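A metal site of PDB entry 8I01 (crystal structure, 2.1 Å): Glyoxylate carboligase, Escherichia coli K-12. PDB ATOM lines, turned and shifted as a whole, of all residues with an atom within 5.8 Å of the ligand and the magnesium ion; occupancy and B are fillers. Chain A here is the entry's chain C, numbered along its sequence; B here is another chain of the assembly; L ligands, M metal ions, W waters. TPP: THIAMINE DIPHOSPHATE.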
ATOM      1  N   ILE A 394     -25.569   2.928  26.356  1.00  0.00           N
ATOM      2  CA  ILE A 394     -24.403   2.936  27.218  1.00  0.00           C
ATOM      3  C   ILE A 394     -23.416   1.889  26.712  1.00  0.00           C
ATOM      4  O   ILE A 394     -23.794   0.911  26.068  1.00  0.00           O
ATOM      5  CB  ILE A 394     -24.781   2.671  28.695  1.00  0.00           C
ATOM      6  CG1 ILE A 394     -23.651   3.123  29.637  1.00  0.00           C
ATOM      7  CG2 ILE A 394     -25.089   1.185  28.919  1.00  0.00           C
ATOM      8  CD1 ILE A 394     -23.919   2.887  31.090  1.00  0.00           C
ATOM      9  N   GLY A 395     -22.145   2.065  27.057  1.00  0.00           N
ATOM     10  CA  GLY A 395     -21.048   1.219  26.616  1.00  0.00           C
ATOM     11  C   GLY A 395     -19.968   2.038  25.917  1.00  0.00           C
ATOM     12  O   GLY A 395     -20.130   3.213  25.615  1.00  0.00           O
ATOM     13  N   LEU A 396     -18.835   1.357  25.663  1.00  0.00           N
ATOM     14  CA  LEU A 396     -17.797   1.995  24.867  1.00  0.00           C
ATOM     15  C   LEU A 396     -18.340   2.394  23.503  1.00  0.00           C
ATOM     16  O   LEU A 396     -17.967   3.452  22.973  1.00  0.00           O
ATOM     17  CB  LEU A 396     -16.594   1.062  24.695  1.00  0.00           C
ATOM     18  CG  LEU A 396     -15.857   0.682  25.973  1.00  0.00           C
ATOM     19  CD1 LEU A 396     -14.636  -0.127  25.674  1.00  0.00           C
ATOM     20  CD2 LEU A 396     -15.481   1.925  26.789  1.00  0.00           C
ATOM     21  N   SER A 397     -19.259   1.595  22.968  1.00  0.00           N
ATOM     22  CA  SER A 397     -19.999   1.934  21.753  1.00  0.00           C
ATOM     23  C   SER A 397     -20.631   3.314  21.858  1.00  0.00           C
ATOM     24  O   SER A 397     -20.513   4.139  20.940  1.00  0.00           O
ATOM     25  CB  SER A 397     -21.101   0.905  21.555  1.00  0.00           C
ATOM     26  OG  SER A 397     -21.812   0.777  22.794  1.00  0.00           O
ATOM     27  N   GLN A 398     -21.346   3.554  22.964  1.00  0.00           N
ATOM     28  CA  GLN A 398     -22.057   4.820  23.174  1.00  0.00           C
ATOM     29  C   GLN A 398     -21.090   5.956  23.491  1.00  0.00           C
ATOM     30  O   GLN A 398     -21.268   7.082  22.994  1.00  0.00           O
ATOM     31  CB  GLN A 398     -23.096   4.658  24.302  1.00  0.00           C
ATOM     32  CG  GLN A 398     -23.886   5.921  24.673  1.00  0.00           C
ATOM     33  CD  GLN A 398     -23.369   6.620  25.942  1.00  0.00           C
ATOM     34  OE1 GLN A 398     -22.503   6.096  26.662  1.00  0.00           O
ATOM     35  NE2 GLN A 398     -23.924   7.819  26.226  1.00  0.00           N
ATOM     36  N   ALA A 419     -29.684   7.124  33.639  1.00  0.00           N
ATOM     37  CA  ALA A 419     -29.906   5.748  34.086  1.00  0.00           C
ATOM     38  C   ALA A 419     -29.194   4.706  33.215  1.00  0.00           C
ATOM     39  O   ALA A 419     -28.668   3.731  33.765  1.00  0.00           O
ATOM     40  CB  ALA A 419     -31.396   5.435  34.142  1.00  0.00           C
ATOM     41  N   GLY A 420     -29.187   4.855  31.891  1.00  0.00           N
ATOM     42  CA  GLY A 420     -28.444   3.951  31.037  1.00  0.00           C
ATOM     43  C   GLY A 420     -28.752   2.449  31.145  1.00  0.00           C
ATOM     44  O   GLY A 420     -27.833   1.643  31.295  1.00  0.00           O
ATOM     45  N   PRO A 421     -30.027   2.045  31.131  1.00  0.00           N
ATOM     46  CA  PRO A 421     -30.348   0.612  31.214  1.00  0.00           C
ATOM     47  C   PRO A 421     -30.032  -0.115  29.915  1.00  0.00           C
ATOM     48  O   PRO A 421     -30.479   0.280  28.840  1.00  0.00           O
ATOM     49  CB  PRO A 421     -31.859   0.600  31.483  1.00  0.00           C
ATOM     50  CG  PRO A 421     -32.355   1.850  30.909  1.00  0.00           C
ATOM     51  CD  PRO A 421     -31.249   2.870  31.064  1.00  0.00           C
ATOM     52  N   LEU A 422     -29.296  -1.222  30.025  1.00  0.00           N
ATOM     53  CA  LEU A 422     -28.992  -2.021  28.845  1.00  0.00           C
ATOM     54  C   LEU A 422     -30.283  -2.571  28.265  1.00  0.00           C
ATOM     55  O   LEU A 422     -31.230  -2.877  28.983  1.00  0.00           O
ATOM     56  CB  LEU A 422     -28.036  -3.175  29.202  1.00  0.00           C
ATOM     57  CG  LEU A 422     -26.587  -2.772  29.468  1.00  0.00           C
ATOM     58  CD1 LEU A 422     -25.811  -3.915  30.132  1.00  0.00           C
ATOM     59  CD2 LEU A 422     -25.914  -2.343  28.154  1.00  0.00           C
ATOM     60  N   SER A 445     -25.519   0.298  19.191  1.00  0.00           N
ATOM     61  CA  SER A 445     -25.404  -0.597  20.340  1.00  0.00           C
ATOM     62  C   SER A 445     -24.115  -1.393  20.253  1.00  0.00           C
ATOM     63  O   SER A 445     -23.657  -1.768  19.162  1.00  0.00           O
ATOM     64  CB  SER A 445     -26.526  -1.640  20.418  1.00  0.00           C
ATOM     65  OG  SER A 445     -27.788  -1.029  20.472  1.00  0.00           O
ATOM     66  N   GLY A 446     -23.557  -1.726  21.445  1.00  0.00           N
ATOM     67  CA  GLY A 446     -22.629  -2.835  21.537  1.00  0.00           C
ATOM     68  C   GLY A 446     -23.363  -4.156  21.539  1.00  0.00           C
ATOM     69  O   GLY A 446     -24.604  -4.185  21.563  1.00  0.00           O
ATOM     70  N   ASP A 447     -22.603  -5.260  21.504  1.00  0.00           N
ATOM     71  CA  ASP A 447     -23.267  -6.560  21.390  1.00  0.00           C
ATOM     72  C   ASP A 447     -24.096  -6.898  22.625  1.00  0.00           C
ATOM     73  O   ASP A 447     -25.189  -7.459  22.508  1.00  0.00           O
ATOM     74  CB  ASP A 447     -22.248  -7.678  21.082  1.00  0.00           C
ATOM     75  CG  ASP A 447     -20.948  -7.579  21.900  1.00  0.00           C
ATOM     76  OD1 ASP A 447     -20.378  -6.472  22.041  1.00  0.00           O
ATOM     77  OD2 ASP A 447     -20.463  -8.646  22.371  1.00  0.00           O
ATOM     78  N   PHE A 448     -23.614  -6.547  23.831  1.00  0.00           N
ATOM     79  CA  PHE A 448     -24.333  -6.926  25.046  1.00  0.00           C
ATOM     80  C   PHE A 448     -25.658  -6.148  25.174  1.00  0.00           C
ATOM     81  O   PHE A 448     -26.716  -6.747  25.395  1.00  0.00           O
ATOM     82  CB  PHE A 448     -23.416  -6.682  26.271  1.00  0.00           C
ATOM     83  CG  PHE A 448     -23.859  -7.389  27.553  1.00  0.00           C
ATOM     84  CD1 PHE A 448     -24.055  -8.756  27.588  1.00  0.00           C
ATOM     85  CD2 PHE A 448     -23.977  -6.670  28.740  1.00  0.00           C
ATOM     86  CE1 PHE A 448     -24.421  -9.409  28.773  1.00  0.00           C
ATOM     87  CE2 PHE A 448     -24.349  -7.291  29.922  1.00  0.00           C
ATOM     88  CZ  PHE A 448     -24.568  -8.678  29.945  1.00  0.00           C
ATOM     89  N   ASP A 449     -25.624  -4.830  24.968  1.00  0.00           N
ATOM     90  CA  ASP A 449     -26.853  -4.040  24.977  1.00  0.00           C
ATOM     91  C   ASP A 449     -27.818  -4.526  23.919  1.00  0.00           C
ATOM     92  O   ASP A 449     -29.036  -4.586  24.150  1.00  0.00           O
ATOM     93  CB  ASP A 449     -26.515  -2.546  24.741  1.00  0.00           C
ATOM     94  CG  ASP A 449     -27.715  -1.704  24.264  1.00  0.00           C
ATOM     95  OD1 ASP A 449     -28.785  -1.696  24.909  1.00  0.00           O
ATOM     96  OD2 ASP A 449     -27.573  -1.010  23.233  1.00  0.00           O
ATOM     97  N   PHE A 450     -27.290  -4.927  22.754  1.00  0.00           N
ATOM     98  CA  PHE A 450     -28.132  -5.412  21.665  1.00  0.00           C
ATOM     99  C   PHE A 450     -28.844  -6.703  22.072  1.00  0.00           C
ATOM    100  O   PHE A 450     -29.974  -6.955  21.636  1.00  0.00           O
ATOM    101  CB  PHE A 450     -27.268  -5.630  20.417  1.00  0.00           C
ATOM    102  CG  PHE A 450     -28.029  -5.936  19.155  1.00  0.00           C
ATOM    103  CD1 PHE A 450     -28.714  -4.950  18.478  1.00  0.00           C
ATOM    104  CD2 PHE A 450     -28.013  -7.211  18.605  1.00  0.00           C
ATOM    105  CE1 PHE A 450     -29.396  -5.239  17.305  1.00  0.00           C
ATOM    106  CE2 PHE A 450     -28.696  -7.497  17.421  1.00  0.00           C
ATOM    107  CZ  PHE A 450     -29.382  -6.510  16.776  1.00  0.00           C
ATOM    108  N   PHE A 452     -29.871  -7.770  25.230  1.00  0.00           N
ATOM    109  CA  PHE A 452     -30.824  -7.748  26.350  1.00  0.00           C
ATOM    110  C   PHE A 452     -32.268  -7.885  25.875  1.00  0.00           C
ATOM    111  O   PHE A 452     -33.040  -8.686  26.406  1.00  0.00           O
ATOM    112  CB  PHE A 452     -30.712  -6.448  27.141  1.00  0.00           C
ATOM    113  CG  PHE A 452     -29.814  -6.522  28.358  1.00  0.00           C
ATOM    114  CD1 PHE A 452     -28.504  -6.960  28.266  1.00  0.00           C
ATOM    115  CD2 PHE A 452     -30.269  -6.071  29.599  1.00  0.00           C
ATOM    116  CE1 PHE A 452     -27.673  -7.008  29.383  1.00  0.00           C
ATOM    117  CE2 PHE A 452     -29.437  -6.120  30.726  1.00  0.00           C
ATOM    118  CZ  PHE A 452     -28.147  -6.585  30.609  1.00  0.00           C
ATOM    119  N   VAL A 472     -21.872  -2.754  16.973  1.00  0.00           N
ATOM    120  CA  VAL A 472     -20.421  -2.855  17.014  1.00  0.00           C
ATOM    121  C   VAL A 472     -20.066  -3.975  17.999  1.00  0.00           C
ATOM    122  O   VAL A 472     -20.275  -3.854  19.217  1.00  0.00           O
ATOM    123  CB  VAL A 472     -19.763  -1.510  17.384  1.00  0.00           C
ATOM    124  CG1 VAL A 472     -19.906  -0.514  16.229  1.00  0.00           C
ATOM    125  CG2 VAL A 472     -20.347  -0.914  18.659  1.00  0.00           C
ATOM    126  N   ASN A 473     -19.543  -5.079  17.471  1.00  0.00           N
ATOM    127  CA  ASN A 473     -19.430  -6.331  18.223  1.00  0.00           C
ATOM    128  C   ASN A 473     -17.972  -6.593  18.578  1.00  0.00           C
ATOM    129  O   ASN A 473     -17.158  -6.927  17.710  1.00  0.00           O
ATOM    130  CB  ASN A 473     -19.997  -7.483  17.394  1.00  0.00           C
ATOM    131  CG  ASN A 473     -19.897  -8.820  18.097  1.00  0.00           C
ATOM    132  OD1 ASN A 473     -19.501  -8.896  19.268  1.00  0.00           O
ATOM    133  ND2 ASN A 473     -20.273  -9.888  17.402  1.00  0.00           N
ATOM    134  N   ASN A 474     -17.636  -6.489  19.866  1.00  0.00           N
ATOM    135  CA  ASN A 474     -16.334  -6.934  20.348  1.00  0.00           C
ATOM    136  C   ASN A 474     -16.422  -8.215  21.174  1.00  0.00           C
ATOM    137  O   ASN A 474     -15.431  -8.606  21.809  1.00  0.00           O
ATOM    138  CB  ASN A 474     -15.665  -5.830  21.168  1.00  0.00           C
ATOM    139  CG  ASN A 474     -16.547  -5.326  22.305  1.00  0.00           C
ATOM    140  OD1 ASN A 474     -17.497  -5.993  22.728  1.00  0.00           O
ATOM    141  ND2 ASN A 474     -16.239  -4.138  22.807  1.00  0.00           N
ATOM    142  N   ALA A 475     -17.588  -8.859  21.230  1.00  0.00           N
ATOM    143  CA  ALA A 475     -17.801 -10.046  22.067  1.00  0.00           C
ATOM    144  C   ALA A 475     -17.311  -9.810  23.504  1.00  0.00           C
ATOM    145  O   ALA A 475     -16.674 -10.676  24.118  1.00  0.00           O
ATOM    146  CB  ALA A 475     -17.123 -11.276  21.446  1.00  0.00           C
ATOM    147  N   TYR A 476     -17.615  -8.630  24.038  1.00  0.00           N
ATOM    148  CA  TYR A 476     -17.119  -8.155  25.321  1.00  0.00           C
ATOM    149  C   TYR A 476     -18.152  -7.220  25.940  1.00  0.00           C
ATOM    150  O   TYR A 476     -18.876  -6.513  25.237  1.00  0.00           O
ATOM    151  CB  TYR A 476     -15.813  -7.340  25.156  1.00  0.00           C
ATOM    152  CG  TYR A 476     -14.513  -7.938  25.687  1.00  0.00           C
ATOM    153  CD1 TYR A 476     -14.246  -7.968  27.044  1.00  0.00           C
ATOM    154  CD2 TYR A 476     -13.536  -8.396  24.819  1.00  0.00           C
ATOM    155  CE1 TYR A 476     -13.051  -8.489  27.520  1.00  0.00           C
ATOM    156  CE2 TYR A 476     -12.325  -8.904  25.275  1.00  0.00           C
ATOM    157  CZ  TYR A 476     -12.093  -8.954  26.641  1.00  0.00           C
ATOM    158  OH  TYR A 476     -10.895  -9.460  27.109  1.00  0.00           O
ATOM    159  N   LEU A 477     -18.189  -7.180  27.279  1.00  0.00           N
ATOM    160  CA  LEU A 477     -18.749  -6.009  27.958  1.00  0.00           C
ATOM    161  C   LEU A 477     -17.616  -4.994  28.048  1.00  0.00           C
ATOM    162  O   LEU A 477     -16.897  -4.928  29.046  1.00  0.00           O
ATOM    163  CB  LEU A 477     -19.296  -6.335  29.344  1.00  0.00           C
ATOM    164  CG  LEU A 477     -19.981  -7.635  29.747  1.00  0.00           C
ATOM    165  CD1 LEU A 477     -20.843  -7.442  31.009  1.00  0.00           C
ATOM    166  CD2 LEU A 477     -20.747  -8.315  28.628  1.00  0.00           C
ATOM    167  N   GLY A 478     -17.438  -4.216  26.990  1.00  0.00           N
ATOM    168  CA  GLY A 478     -16.179  -3.486  26.831  1.00  0.00           C
ATOM    169  C   GLY A 478     -15.978  -2.417  27.881  1.00  0.00           C
ATOM    170  O   GLY A 478     -14.875  -2.248  28.404  1.00  0.00           O
ATOM    171  N   LEU A 479     -17.042  -1.678  28.224  1.00  0.00           N
ATOM    172  CA  LEU A 479     -16.879  -0.643  29.239  1.00  0.00           C
ATOM    173  C   LEU A 479     -16.496  -1.256  30.580  1.00  0.00           C
ATOM    174  O   LEU A 479     -15.678  -0.687  31.310  1.00  0.00           O
ATOM    175  CB  LEU A 479     -18.161   0.184  29.353  1.00  0.00           C
ATOM    176  CG  LEU A 479     -18.178   1.282  30.440  1.00  0.00           C
ATOM    177  CD1 LEU A 479     -16.974   2.187  30.345  1.00  0.00           C
ATOM    178  CD2 LEU A 479     -19.431   2.105  30.324  1.00  0.00           C
ATOM    179  N   ILE A 480     -17.059  -2.418  30.920  1.00  0.00           N
ATOM    180  CA  ILE A 480     -16.725  -3.043  32.212  1.00  0.00           C
ATOM    181  C   ILE A 480     -15.304  -3.592  32.187  1.00  0.00           C
ATOM    182  O   ILE A 480     -14.584  -3.528  33.195  1.00  0.00           O
ATOM    183  CB  ILE A 480     -17.749  -4.136  32.578  1.00  0.00           C
ATOM    184  CG1 ILE A 480     -19.181  -3.602  32.425  1.00  0.00           C
ATOM    185  CG2 ILE A 480     -17.554  -4.603  34.009  1.00  0.00           C
ATOM    186  CD1 ILE A 480     -19.411  -2.169  32.967  1.00  0.00           C
ATOM    187  N   LEU A 495     -17.989 -12.479  26.153  1.00  0.00           N
ATOM    188  CA  LEU A 495     -19.163 -13.151  25.608  1.00  0.00           C
ATOM    189  C   LEU A 495     -18.829 -14.168  24.521  1.00  0.00           C
ATOM    190  O   LEU A 495     -19.742 -14.801  23.981  1.00  0.00           O
ATOM    191  CB  LEU A 495     -20.140 -12.125  25.039  1.00  0.00           C
ATOM    192  CG  LEU A 495     -20.640 -11.154  26.111  1.00  0.00           C
ATOM    193  CD1 LEU A 495     -21.373  -9.967  25.494  1.00  0.00           C
ATOM    194  CD2 LEU A 495     -21.541 -11.917  27.073  1.00  0.00           C
ATOM    195  N   VAL B  26     -24.363  -9.827  36.283  1.00  0.00           N
ATOM    196  CA  VAL B  26     -23.882  -8.918  35.268  1.00  0.00           C
ATOM    197  C   VAL B  26     -23.033  -7.878  35.975  1.00  0.00           C
ATOM    198  O   VAL B  26     -23.561  -7.061  36.748  1.00  0.00           O
ATOM    199  CB  VAL B  26     -25.033  -8.251  34.502  1.00  0.00           C
ATOM    200  CG1 VAL B  26     -24.460  -7.194  33.542  1.00  0.00           C
ATOM    201  CG2 VAL B  26     -25.853  -9.304  33.769  1.00  0.00           C
ATOM    202  N   PRO B  27     -21.723  -7.866  35.756  1.00  0.00           N
ATOM    203  CA  PRO B  27     -20.861  -6.893  36.437  1.00  0.00           C
ATOM    204  C   PRO B  27     -21.035  -5.483  35.880  1.00  0.00           C
ATOM    205  O   PRO B  27     -21.595  -5.241  34.812  1.00  0.00           O
ATOM    206  CB  PRO B  27     -19.457  -7.446  36.177  1.00  0.00           C
ATOM    207  CG  PRO B  27     -19.586  -8.182  34.885  1.00  0.00           C
ATOM    208  CD  PRO B  27     -20.955  -8.775  34.879  1.00  0.00           C
ATOM    209  N   GLY B  28     -20.572  -4.524  36.676  1.00  0.00           N
ATOM    210  CA  GLY B  28     -20.545  -3.119  36.305  1.00  0.00           C
ATOM    211  C   GLY B  28     -19.583  -2.399  37.219  1.00  0.00           C
ATOM    212  O   GLY B  28     -19.106  -2.963  38.213  1.00  0.00           O
ATOM    213  N   ALA B  29     -19.335  -1.124  36.892  1.00  0.00           N
ATOM    214  CA  ALA B  29     -18.317  -0.373  37.623  1.00  0.00           C
ATOM    215  C   ALA B  29     -18.594  -0.352  39.133  1.00  0.00           C
ATOM    216  O   ALA B  29     -17.682  -0.549  39.932  1.00  0.00           O
ATOM    217  CB  ALA B  29     -18.229   1.050  37.086  1.00  0.00           C
ATOM    218  N   VAL B  52     -30.057  -8.695  33.134  1.00  0.00           N
ATOM    219  CA  VAL B  52     -30.067  -8.758  34.602  1.00  0.00           C
ATOM    220  C   VAL B  52     -31.303  -9.503  35.074  1.00  0.00           C
ATOM    221  O   VAL B  52     -31.238 -10.270  36.040  1.00  0.00           O
ATOM    222  CB  VAL B  52     -29.980  -7.358  35.231  1.00  0.00           C
ATOM    223  CG1 VAL B  52     -30.347  -7.423  36.720  1.00  0.00           C
ATOM    224  CG2 VAL B  52     -28.583  -6.765  35.030  1.00  0.00           C
ATOM    225  N   THR B  76     -24.912  -4.279  39.048  1.00  0.00           N
ATOM    226  CA  THR B  76     -24.328  -2.986  39.383  1.00  0.00           C
ATOM    227  C   THR B  76     -25.399  -2.063  39.972  1.00  0.00           C
ATOM    228  O   THR B  76     -26.446  -2.539  40.445  1.00  0.00           O
ATOM    229  CB  THR B  76     -23.642  -2.363  38.142  1.00  0.00           C
ATOM    230  OG1 THR B  76     -22.835  -1.247  38.530  1.00  0.00           O
ATOM    231  CG2 THR B  76     -24.671  -1.903  37.093  1.00  0.00           C
ATOM    232  N   PRO B  79     -30.067   0.862  37.125  1.00  0.00           N
ATOM    233  CA  PRO B  79     -31.054   0.005  36.419  1.00  0.00           C
ATOM    234  C   PRO B  79     -30.906  -1.498  36.670  1.00  0.00           C
ATOM    235  O   PRO B  79     -31.871  -2.241  36.440  1.00  0.00           O
ATOM    236  CB  PRO B  79     -30.825   0.343  34.941  1.00  0.00           C
ATOM    237  CG  PRO B  79     -29.404   0.771  34.885  1.00  0.00           C
ATOM    238  CD  PRO B  79     -29.154   1.533  36.182  1.00  0.00           C
ATOM    239  N   ALA B  80     -29.713  -1.989  37.029  1.00  0.00           N
ATOM    240  CA  ALA B  80     -29.608  -3.408  37.354  1.00  0.00           C
ATOM    241  C   ALA B  80     -30.486  -3.759  38.549  1.00  0.00           C
ATOM    242  O   ALA B  80     -31.181  -4.778  38.531  1.00  0.00           O
ATOM    243  CB  ALA B  80     -28.151  -3.797  37.619  1.00  0.00           C
ATOM    244  N   ASP B  83     -34.051  -3.844  37.457  1.00  0.00           N
ATOM    245  CA  ASP B  83     -34.311  -5.050  36.680  1.00  0.00           C
ATOM    246  C   ASP B  83     -34.512  -6.287  37.556  1.00  0.00           C
ATOM    247  O   ASP B  83     -34.914  -7.333  37.033  1.00  0.00           O
ATOM    248  CB  ASP B  83     -33.161  -5.338  35.720  1.00  0.00           C
ATOM    249  CG  ASP B  83     -33.208  -4.484  34.463  1.00  0.00           C
ATOM    250  OD1 ASP B  83     -34.220  -3.800  34.202  1.00  0.00           O
ATOM    251  OD2 ASP B  83     -32.195  -4.507  33.718  1.00  0.00           O
ATOM    252  N   GLN B 116     -26.461   6.898  37.747  1.00  0.00           N
ATOM    253  CA  GLN B 116     -27.015   5.567  37.998  1.00  0.00           C
ATOM    254  C   GLN B 116     -27.163   5.267  39.487  1.00  0.00           C
ATOM    255  O   GLN B 116     -26.973   4.141  39.921  1.00  0.00           O
ATOM    256  CB  GLN B 116     -26.172   4.479  37.332  1.00  0.00           C
ATOM    257  CG  GLN B 116     -26.456   4.301  35.858  1.00  0.00           C
ATOM    258  CD  GLN B 116     -25.804   3.055  35.288  1.00  0.00           C
ATOM    259  OE1 GLN B 116     -24.832   2.550  35.838  1.00  0.00           O
ATOM    260  NE2 GLN B 116     -26.351   2.542  34.175  1.00  0.00           N
HETATM  261  N1' TPP L   1     -26.755  -3.864  33.971  1.00  0.00           N
HETATM  262  C2' TPP L   1     -27.669  -3.009  33.472  1.00  0.00           C
HETATM  263  CM2 TPP L   1     -29.101  -3.415  33.513  1.00  0.00           C
HETATM  264  N3' TPP L   1     -27.398  -1.814  32.930  1.00  0.00           N
HETATM  265  C4' TPP L   1     -26.103  -1.427  32.876  1.00  0.00           C
HETATM  266  N4' TPP L   1     -25.855  -0.231  32.326  1.00  0.00           N
HETATM  267  C5' TPP L   1     -25.059  -2.272  33.366  1.00  0.00           C
HETATM  268  C6' TPP L   1     -25.473  -3.471  33.910  1.00  0.00           C
HETATM  269  C7' TPP L   1     -23.592  -1.893  33.368  1.00  0.00           C
HETATM  270  N3  TPP L   1     -22.994  -1.758  32.017  1.00  0.00           N
HETATM  271  C2  TPP L   1     -22.763  -0.595  31.430  1.00  0.00           C
HETATM  272  S1  TPP L   1     -22.030  -0.766  29.927  1.00  0.00           S
HETATM  273  C5  TPP L   1     -21.993  -2.487  30.089  1.00  0.00           C
HETATM  274  C4  TPP L   1     -22.543  -2.866  31.279  1.00  0.00           C
HETATM  275  CM4 TPP L   1     -22.705  -4.253  31.800  1.00  0.00           C
HETATM  276  C6  TPP L   1     -21.442  -3.358  29.004  1.00  0.00           C
HETATM  277  C7  TPP L   1     -21.706  -2.800  27.619  1.00  0.00           C
HETATM  278  O7  TPP L   1     -21.467  -3.833  26.629  1.00  0.00           O
HETATM  279  PA  TPP L   1     -21.757  -3.641  25.094  1.00  0.00           P
HETATM  280  O1A TPP L   1     -23.200  -3.170  24.898  1.00  0.00           O
HETATM  281  O2A TPP L   1     -21.316  -4.840  24.337  1.00  0.00           O
HETATM  282  O3A TPP L   1     -20.775  -2.423  24.831  1.00  0.00           O
HETATM  283  PB  TPP L   1     -19.210  -2.168  24.704  1.00  0.00           P
HETATM  284  O1B TPP L   1     -18.506  -3.492  24.615  1.00  0.00           O
HETATM  285  O2B TPP L   1     -19.066  -1.313  23.420  1.00  0.00           O
HETATM  286  O3B TPP L   1     -18.823  -1.388  25.982  1.00  0.00           O
HETATM  287 MG    MG M   1     -19.316  -5.238  23.512  1.00  0.00          MG
HETATM  288  O   HOH W   1     -23.152   1.275  33.924  1.00  0.00           O
HETATM  289  O   HOH W   2     -17.047  -0.747  21.356  1.00  0.00           O
HETATM  290  O   HOH W   3     -25.573  -5.374  36.481  1.00  0.00           O
HETATM  291  O   HOH W   4     -19.472  -3.734  21.946  1.00  0.00           O
HETATM  292  O   HOH W   5     -23.714  -0.937  23.936  1.00  0.00           O
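The backbone NH of Asp 447 sits close to an oxygen (O2A) of the ligand (3.1 Å).
O3B of the ligand is in hydrogen-bond range of N of Gly 478, 3.3 Å away.
The backbone NH of Leu 396 sits at hydrogen-bond distance from an oxygen (O3B) of the ligand (2.8 Å).
The backbone NH of Leu 479 is in hydrogen-bond range of an oxygen (O3B) of the ligand, 2.9 Å away.
The backbone NH of Phe 448 sits close to an oxygen (O2A) of the ligand, at 2.9 Å.
A nitrogen (N4') of the ligand lies within hydrogen-bond range of the backbone carbonyl oxygen of Gly 420.
N of Asp 449 is in hydrogen-bond range of O1A of the ligand (2.9 Å).
The backbone NH (N) of Ser 397 is in hydrogen-bond range of an oxygen (O2B) of the ligand, 2.9 Å away.
A nitrogen (N4') of the ligand lies close to the side-chain amide nitrogen (NE2) of Gln 116 of chain B (3.4 Å).
The backbone NH (N) of Ala 475 lies close to the side-chain carboxylate (OD2) of Asp 447 (3.1 Å).
The side-chain carboxylate (OD2) of Asp 447 sits close to the side-chain amide oxygen (OD1) of Asn 473, at 3.3 Å.
The backbone carbonyl oxygen (O) of Gly 420 lies within hydrogen-bond range of the side-chain amide nitrogen (NE2) of Gln 116 of chain B (3.4 Å).
The side-chain hydroxyl of Ser 445 is in hydrogen-bond range of the side-chain carboxylate of Asp 449 (2.8 Å).
The backbone NH (N) of Gly 446 sits at hydrogen-bond distance from the side-chain hydroxyl (OG) of Ser 397 (3.3 Å).
NE2 of Gln 116 of chain B sits at hydrogen-bond distance from O of Ala 419, at 2.6 Å.
Merely in contact with the ligand: Ile 394 (3.7 Å), Gly 395 (3.5 Å), Leu 422 (3.5 Å), Gly 446 (3.4 Å), Phe 452 (3.9 Å), Leu 477 (3.7 Å), Ile 480 (3.6 Å), Val 26 of chain B (3.8 Å), Pro 27 of chain B (3.4 Å), Val 52 of chain B (3.6 Å), Thr 76 of chain B (3.6 Å), Pro 79 of chain B (3.8 Å), Ala 80 of chain B (3.8 Å) and Asp 83 of chain B (3.3 Å).
Hydrophobic or aromatic side chains that line the ligand: Ile 394, Leu 396, Leu 422, Phe 448, Phe 452, Leu 477, Leu 479, Ile 480, Val 26 of chain B, Val 52 of chain B, Pro 79 of chain B and Ala 80 of chain B.
Of the 36 residues printed, 25 come within 4 Å of the ligand.
The nearest printed residue that does not touch the ligand is Pro 421 (4.2 Å).
The nearest printed residue that does not touch the magnesium ion is Gly 478 (4.1 Å).
The magnesium ion is bound by the side-chain amide oxygen (OD1) of Asn 474.
The magnesium ion is bound by water W4.
The magnesium ion is bound by O of Tyr 476 (2.2 Å).
The magnesium ion is bound by OD1 of Asp 447 (2.2 Å).
An oxygen (O2A) of the ligand is bound to the magnesium ion, 2.2 Å away.
The magnesium ion is bound by O1B of the ligand.
The magnesium ion has six donor atoms within binding distance.
Water W4 lies within hydrogen-bond range of O of Val 472 (2.8 Å), O2B of the ligand (2.9 Å) and ND2 of Asn 474 (3.4 Å).
Water W5 lies within hydrogen-bond range of an oxygen (O1A) of the ligand (2.5 Å), the backbone NH (N) of Gly 446 (2.6 Å), the side-chain hydroxyl (OG) of Ser 397 (2.8 Å) and the backbone carbonyl oxygen (O) of Ile 394 (2.8 Å).
Water W1 bridges OE1 of Gln 116 of chain B (2.8 Å) and N4' of the ligand (3.5 Å).
Water W3 lies within hydrogen-bond range of O of Val 26 of chain B, N of Thr 76 of chain B and N1' of the ligand.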
